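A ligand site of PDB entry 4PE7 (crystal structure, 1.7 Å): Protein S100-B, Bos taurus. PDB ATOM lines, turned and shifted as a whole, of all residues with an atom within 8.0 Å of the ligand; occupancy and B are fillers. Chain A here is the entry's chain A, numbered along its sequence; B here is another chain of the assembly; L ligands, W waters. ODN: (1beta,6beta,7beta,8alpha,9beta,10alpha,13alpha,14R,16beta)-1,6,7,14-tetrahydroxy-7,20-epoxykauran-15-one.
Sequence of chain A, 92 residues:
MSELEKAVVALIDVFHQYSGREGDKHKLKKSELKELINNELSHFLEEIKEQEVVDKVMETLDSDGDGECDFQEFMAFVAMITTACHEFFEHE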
ATOM      1  N   LEU A  41      -9.207 -13.061  13.066  1.00  0.00           N
ATOM      2  CA  LEU A  41      -9.116 -11.821  13.836  1.00  0.00           C
ATOM      3  C   LEU A  41      -8.052 -11.952  14.918  1.00  0.00           C
ATOM      4  O   LEU A  41      -8.144 -11.340  15.991  1.00  0.00           O
ATOM      5  CB  LEU A  41     -10.478 -11.469  14.453  1.00  0.00           C
ATOM      6  CG  LEU A  41     -11.546 -11.031  13.451  1.00  0.00           C
ATOM      7  CD1 LEU A  41     -12.941 -11.058  14.072  1.00  0.00           C
ATOM      8  CD2 LEU A  41     -11.217  -9.634  12.906  1.00  0.00           C
ATOM      9  N   SER A  42      -7.021 -12.743  14.620  1.00  0.00           N
ATOM     10  CA  SER A  42      -5.973 -13.067  15.602  1.00  0.00           C
ATOM     11  C   SER A  42      -5.146 -11.848  16.032  1.00  0.00           C
ATOM     12  O   SER A  42      -4.461 -11.908  17.065  1.00  0.00           O
ATOM     13  CB  SER A  42      -5.032 -14.143  15.049  1.00  0.00           C
ATOM     14  OG  SER A  42      -4.255 -13.645  13.964  1.00  0.00           O
ATOM     15  N   HIS A  43      -5.195 -10.764  15.268  1.00  0.00           N
ATOM     16  CA  HIS A  43      -4.449  -9.551  15.650  1.00  0.00           C
ATOM     17  C   HIS A  43      -5.333  -8.511  16.344  1.00  0.00           C
ATOM     18  O   HIS A  43      -4.820  -7.545  16.933  1.00  0.00           O
ATOM     19  CB  HIS A  43      -3.757  -8.927  14.441  1.00  0.00           C
ATOM     20  CG  HIS A  43      -2.960  -9.900  13.623  1.00  0.00           C
ATOM     21  ND1 HIS A  43      -1.711 -10.367  14.010  1.00  0.00           N
ATOM     22  CD2 HIS A  43      -3.235 -10.514  12.454  1.00  0.00           C
ATOM     23  CE1 HIS A  43      -1.256 -11.217  13.103  1.00  0.00           C
ATOM     24  NE2 HIS A  43      -2.169 -11.322  12.140  1.00  0.00           N
ATOM     25  N   PHE A  44      -6.645  -8.701  16.287  1.00  0.00           N
ATOM     26  CA  PHE A  44      -7.594  -7.736  16.852  1.00  0.00           C
ATOM     27  C   PHE A  44      -8.255  -8.229  18.134  1.00  0.00           C
ATOM     28  O   PHE A  44      -8.552  -7.438  19.025  1.00  0.00           O
ATOM     29  CB  PHE A  44      -8.695  -7.383  15.834  1.00  0.00           C
ATOM     30  CG  PHE A  44      -8.217  -6.545  14.679  1.00  0.00           C
ATOM     31  CD1 PHE A  44      -6.945  -5.984  14.680  1.00  0.00           C
ATOM     32  CD2 PHE A  44      -9.037  -6.320  13.580  1.00  0.00           C
ATOM     33  CE1 PHE A  44      -6.515  -5.208  13.608  1.00  0.00           C
ATOM     34  CE2 PHE A  44      -8.621  -5.547  12.507  1.00  0.00           C
ATOM     35  CZ  PHE A  44      -7.342  -4.989  12.520  1.00  0.00           C
ATOM     36  N   LEU A  45      -8.525  -9.528  18.204  1.00  0.00           N
ATOM     37  CA  LEU A  45      -9.212 -10.108  19.347  1.00  0.00           C
ATOM     38  C   LEU A  45      -8.357 -11.203  19.990  1.00  0.00           C
ATOM     39  O   LEU A  45      -7.643 -11.939  19.291  1.00  0.00           O
ATOM     40  CB  LEU A  45     -10.565 -10.697  18.929  1.00  0.00           C
ATOM     41  CG  LEU A  45     -11.579  -9.689  18.393  1.00  0.00           C
ATOM     42  CD1 LEU A  45     -12.866 -10.379  17.948  1.00  0.00           C
ATOM     43  CD2 LEU A  45     -11.883  -8.670  19.468  1.00  0.00           C
ATOM     44  N   GLU A  46      -8.431 -11.316  21.300  1.00  0.00           N
ATOM     45  CA  GLU A  46      -7.733 -12.381  21.990  1.00  0.00           C
ATOM     46  C   GLU A  46      -8.311 -13.719  21.558  1.00  0.00           C
ATOM     47  O   GLU A  46      -9.527 -13.860  21.404  1.00  0.00           O
ATOM     48  CB  GLU A  46      -7.861 -12.215  23.501  1.00  0.00           C
ATOM     49  CG  GLU A  46      -6.996 -13.189  24.284  1.00  0.00           C
ATOM     50  CD  GLU A  46      -7.062 -12.959  25.772  1.00  0.00           C
ATOM     51  OE1 GLU A  46      -7.180 -11.794  26.190  1.00  0.00           O
ATOM     52  OE2 GLU A  46      -6.992 -13.958  26.518  1.00  0.00           O
ATOM     53  N   MET A  80     -18.750  -3.198  14.963  1.00  0.00           N
ATOM     54  CA  MET A  80     -18.225  -3.027  16.317  1.00  0.00           C
ATOM     55  C   MET A  80     -16.699  -2.959  16.300  1.00  0.00           C
ATOM     56  O   MET A  80     -16.093  -2.062  16.891  1.00  0.00           O
ATOM     57  CB  MET A  80     -18.616  -4.219  17.196  1.00  0.00           C
ATOM     58  CG  MET A  80     -20.086  -4.291  17.584  1.00  0.00           C
ATOM     59  SD  MET A  80     -20.401  -5.869  18.411  1.00  0.00           S
ATOM     60  CE  MET A  80     -18.914  -6.001  19.396  1.00  0.00           C
ATOM     61  N   ILE A  81     -16.092  -3.942  15.645  1.00  0.00           N
ATOM     62  CA  ILE A  81     -14.637  -4.030  15.560  1.00  0.00           C
ATOM     63  C   ILE A  81     -14.050  -2.836  14.815  1.00  0.00           C
ATOM     64  O   ILE A  81     -13.116  -2.175  15.290  1.00  0.00           O
ATOM     65  CB  ILE A  81     -14.185  -5.339  14.867  1.00  0.00           C
ATOM     66  CG1 ILE A  81     -14.632  -6.551  15.687  1.00  0.00           C
ATOM     67  CG2 ILE A  81     -12.658  -5.342  14.692  1.00  0.00           C
ATOM     68  CD1 ILE A  81     -14.583  -7.867  14.917  1.00  0.00           C
ATOM     69  N   THR A  82     -14.603  -2.533  13.648  1.00  0.00           N
ATOM     70  CA  THR A  82     -14.089  -1.441  12.829  1.00  0.00           C
ATOM     71  C   THR A  82     -14.217  -0.091  13.537  1.00  0.00           C
ATOM     72  O   THR A  82     -13.320   0.753  13.467  1.00  0.00           O
ATOM     73  CB  THR A  82     -14.818  -1.396  11.488  1.00  0.00           C
ATOM     74  OG1 THR A  82     -14.798  -2.703  10.897  1.00  0.00           O
ATOM     75  CG2 THR A  82     -14.137  -0.400  10.570  1.00  0.00           C
ATOM     76  N   THR A  83     -15.338   0.105  14.231  1.00  0.00           N
ATOM     77  CA  THR A  83     -15.551   1.351  14.980  1.00  0.00           C
ATOM     78  C   THR A  83     -14.538   1.486  16.106  1.00  0.00           C
ATOM     79  O   THR A  83     -13.971   2.562  16.320  1.00  0.00           O
ATOM     80  CB  THR A  83     -16.977   1.448  15.521  1.00  0.00           C
ATOM     81  OG1 THR A  83     -17.900   1.468  14.418  1.00  0.00           O
ATOM     82  CG2 THR A  83     -17.145   2.714  16.352  1.00  0.00           C
ATOM     83  N   ALA A  84     -14.298   0.402  16.847  1.00  0.00           N
ATOM     84  CA  ALA A  84     -13.268   0.392  17.885  1.00  0.00           C
ATOM     85  C   ALA A  84     -11.905   0.769  17.306  1.00  0.00           C
ATOM     86  O   ALA A  84     -11.190   1.602  17.883  1.00  0.00           O
ATOM     87  CB  ALA A  84     -13.192  -0.988  18.543  1.00  0.00           C
ATOM     88  N   CYS A  85     -11.539   0.156  16.187  1.00  0.00           N
ATOM     89  CA  CYS A  85     -10.258   0.471  15.543  1.00  0.00           C
ATOM     90  C   CYS A  85     -10.205   1.887  14.975  1.00  0.00           C
ATOM     91  O   CYS A  85      -9.176   2.563  15.064  1.00  0.00           O
ATOM     92  CB  CYS A  85      -9.928  -0.573  14.479  1.00  0.00           C
ATOM     93  SG  CYS A  85      -9.640  -2.218  15.137  1.00  0.00           S
ATOM     94  N   HIS A  86     -11.316   2.348  14.391  1.00  0.00           N
ATOM     95  CA  HIS A  86     -11.403   3.733  13.901  1.00  0.00           C
ATOM     96  C   HIS A  86     -11.095   4.699  15.042  1.00  0.00           C
ATOM     97  O   HIS A  86     -10.273   5.601  14.890  1.00  0.00           O
ATOM     98  CB  HIS A  86     -12.797   4.009  13.327  1.00  0.00           C
ATOM     99  CG  HIS A  86     -13.125   5.468  13.189  1.00  0.00           C
ATOM    100  ND1 HIS A  86     -12.674   6.235  12.136  1.00  0.00           N
ATOM    101  CD2 HIS A  86     -13.866   6.293  13.964  1.00  0.00           C
ATOM    102  CE1 HIS A  86     -13.118   7.474  12.282  1.00  0.00           C
ATOM    103  NE2 HIS A  86     -13.842   7.533  13.383  1.00  0.00           N
ATOM    104  N   GLU A  87     -11.754   4.494  16.176  1.00  0.00           N
ATOM    105  CA  GLU A  87     -11.544   5.362  17.334  1.00  0.00           C
ATOM    106  C   GLU A  87     -10.112   5.273  17.877  1.00  0.00           C
ATOM    107  O   GLU A  87      -9.521   6.282  18.267  1.00  0.00           O
ATOM    108  CB  GLU A  87     -12.553   5.036  18.444  1.00  0.00           C
ATOM    109  CG  GLU A  87     -13.990   5.467  18.119  1.00  0.00           C
ATOM    110  CD  GLU A  87     -15.005   4.940  19.110  1.00  0.00           C
ATOM    111  OE1 GLU A  87     -16.216   5.182  18.927  1.00  0.00           O
ATOM    112  OE2 GLU A  87     -14.597   4.266  20.084  1.00  0.00           O
ATOM    113  N   PHE A  88      -9.567   4.064  17.893  1.00  0.00           N
ATOM    114  CA  PHE A  88      -8.186   3.836  18.296  1.00  0.00           C
ATOM    115  C   PHE A  88      -7.198   4.566  17.374  1.00  0.00           C
ATOM    116  O   PHE A  88      -6.336   5.305  17.838  1.00  0.00           O
ATOM    117  CB  PHE A  88      -7.879   2.331  18.305  1.00  0.00           C
ATOM    118  CG  PHE A  88      -6.460   1.997  18.678  1.00  0.00           C
ATOM    119  CD1 PHE A  88      -5.622   1.374  17.768  1.00  0.00           C
ATOM    120  CD2 PHE A  88      -5.965   2.331  19.940  1.00  0.00           C
ATOM    121  CE1 PHE A  88      -4.313   1.064  18.110  1.00  0.00           C
ATOM    122  CE2 PHE A  88      -4.656   2.022  20.282  1.00  0.00           C
ATOM    123  CZ  PHE A  88      -3.822   1.386  19.371  1.00  0.00           C
ATOM    124  N   PHE A  89      -7.351   4.365  16.061  1.00  0.00           N
ATOM    125  CA  PHE A  89      -6.410   4.922  15.095  1.00  0.00           C
ATOM    126  C   PHE A  89      -6.553   6.434  14.886  1.00  0.00           C
ATOM    127  O   PHE A  89      -5.577   7.106  14.534  1.00  0.00           O
ATOM    128  CB  PHE A  89      -6.511   4.181  13.755  1.00  0.00           C
ATOM    129  CG  PHE A  89      -5.961   2.788  13.796  1.00  0.00           C
ATOM    130  CD1 PHE A  89      -4.642   2.563  14.158  1.00  0.00           C
ATOM    131  CD2 PHE A  89      -6.750   1.696  13.450  1.00  0.00           C
ATOM    132  CE1 PHE A  89      -4.121   1.275  14.206  1.00  0.00           C
ATOM    133  CE2 PHE A  89      -6.241   0.407  13.480  1.00  0.00           C
ATOM    134  CZ  PHE A  89      -4.919   0.194  13.861  1.00  0.00           C
ATOM    135  N   GLU B   5      -9.054  -8.799   8.383  1.00  0.00           N
ATOM    136  CA  GLU B   5      -8.395  -7.686   9.086  1.00  0.00           C
ATOM    137  C   GLU B   5      -8.018  -6.562   8.135  1.00  0.00           C
ATOM    138  O   GLU B   5      -8.182  -5.370   8.453  1.00  0.00           O
ATOM    139  CB  GLU B   5      -7.170  -8.228   9.841  1.00  0.00           C
ATOM    140  CG  GLU B   5      -7.582  -8.999  11.072  1.00  0.00           C
ATOM    141  CD  GLU B   5      -6.456  -9.806  11.684  1.00  0.00           C
ATOM    142  OE1 GLU B   5      -5.510 -10.156  10.949  1.00  0.00           O
ATOM    143  OE2 GLU B   5      -6.534 -10.091  12.884  1.00  0.00           O
ATOM    144  N   VAL B   8     -11.066  -4.528   7.399  1.00  0.00           N
ATOM    145  CA  VAL B   8     -11.381  -3.595   8.471  1.00  0.00           C
ATOM    146  C   VAL B   8     -10.546  -2.332   8.330  1.00  0.00           C
ATOM    147  O   VAL B   8     -11.061  -1.221   8.418  1.00  0.00           O
ATOM    148  CB  VAL B   8     -11.161  -4.243   9.862  1.00  0.00           C
ATOM    149  CG1 VAL B   8     -11.159  -3.181  10.980  1.00  0.00           C
ATOM    150  CG2 VAL B   8     -12.232  -5.292  10.119  1.00  0.00           C
ATOM    151  N   VAL B   9      -9.252  -2.513   8.089  1.00  0.00           N
ATOM    152  CA  VAL B   9      -8.352  -1.363   7.961  1.00  0.00           C
ATOM    153  C   VAL B   9      -8.698  -0.535   6.721  1.00  0.00           C
ATOM    154  O   VAL B   9      -8.668   0.700   6.775  1.00  0.00           O
ATOM    155  CB  VAL B   9      -6.878  -1.804   7.950  1.00  0.00           C
ATOM    156  CG1 VAL B   9      -5.957  -0.623   7.635  1.00  0.00           C
ATOM    157  CG2 VAL B   9      -6.506  -2.421   9.299  1.00  0.00           C
ATOM    158  N   ILE B  12     -11.557   1.842   7.448  1.00  0.00           N
ATOM    159  CA  ILE B  12     -11.084   2.978   8.230  1.00  0.00           C
ATOM    160  C   ILE B  12     -10.291   3.922   7.316  1.00  0.00           C
ATOM    161  O   ILE B  12     -10.508   5.138   7.335  1.00  0.00           O
ATOM    162  CB  ILE B  12     -10.235   2.484   9.423  1.00  0.00           C
ATOM    163  CG1 ILE B  12     -11.112   1.710  10.403  1.00  0.00           C
ATOM    164  CG2 ILE B  12      -9.558   3.651  10.132  1.00  0.00           C
ATOM    165  CD1 ILE B  12     -10.345   0.759  11.325  1.00  0.00           C
HETATM  166  O3  ODN L   1      -5.437  -2.378  17.296  1.00  0.00           O
HETATM  167  C17 ODN L   1      -6.504  -2.737  17.780  1.00  0.00           C
HETATM  168  C10 ODN L   1      -6.708  -3.072  19.238  1.00  0.00           C
HETATM  169  C18 ODN L   1      -5.675  -3.973  19.949  1.00  0.00           C
HETATM  170  O4  ODN L   1      -5.395  -5.130  19.156  1.00  0.00           O
HETATM  171  O1  ODN L   1      -6.258  -4.367  21.200  1.00  0.00           O
HETATM  172  C8  ODN L   1      -6.669  -3.270  22.040  1.00  0.00           C
HETATM  173  C19 ODN L   1      -4.373  -3.266  20.281  1.00  0.00           C
HETATM  174  O5  ODN L   1      -3.652  -2.901  19.086  1.00  0.00           O
HETATM  175  C6  ODN L   1      -4.654  -2.026  21.134  1.00  0.00           C
HETATM  176  C3  ODN L   1      -3.688  -1.915  22.346  1.00  0.00           C
HETATM  177  C5  ODN L   1      -2.296  -1.665  21.805  1.00  0.00           C
HETATM  178  C4  ODN L   1      -3.599  -3.182  23.208  1.00  0.00           C
HETATM  179  C2  ODN L   1      -4.089  -0.723  23.185  1.00  0.00           C
HETATM  180  C1  ODN L   1      -5.542  -0.828  23.612  1.00  0.00           C
HETATM  181  C13 ODN L   1      -7.770  -2.902  16.972  1.00  0.00           C
HETATM  182  C14 ODN L   1      -8.078  -1.753  16.004  1.00  0.00           C
HETATM  183  C12 ODN L   1      -8.780  -2.946  18.102  1.00  0.00           C
HETATM  184  C11 ODN L   1      -8.065  -3.774  19.141  1.00  0.00           C
HETATM  185  O2  ODN L   1      -7.887  -5.113  18.694  1.00  0.00           O
HETATM  186  C15 ODN L   1      -8.984  -1.539  18.669  1.00  0.00           C
HETATM  187  C16 ODN L   1      -8.295  -1.326  20.035  1.00  0.00           C
HETATM  188  C9  ODN L   1      -6.835  -1.780  20.046  1.00  0.00           C
HETATM  189  C7  ODN L   1      -6.165  -1.953  21.439  1.00  0.00           C
HETATM  190  C   ODN L   1      -6.463  -0.795  22.393  1.00  0.00           C
HETATM  191  O   ODN L   1      -7.807  -0.870  22.903  1.00  0.00           O
HETATM  192  O   HOH W   1      -9.054  -6.909  21.457  1.00  0.00           O
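The side-chain sulfur of Cys 85 is covalently linked to a carbon (C14) of the ligand (1.8 Å). An oxygen (O2) of the ligand is in hydrogen-bond range of the backbone carbonyl oxygen (O) of Phe 44, at 2.4 Å. O4 of the ligand is in hydrogen-bond range of O of His 43 (3.3 Å).
The side-chain carboxylate (OE2) of Glu 5 of chain B sits at hydrogen-bond distance from the backbone NH (N) of His 43 (2.8 Å).
Ala 84 touches the ligand. Phe 88 touches the ligand (CE1 to O3, 3.7 Å). Phe 89 touches the ligand (CE2 to C14, 3.8 Å). Within 4 Å of the ligand: His 43, Phe 44, Ala 84, Cys 85, Phe 88 and Phe 89.
Water W1 lies within hydrogen-bond range of O of Phe 44 (2.5 Å) and O2 of the ligand (3.5 Å).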
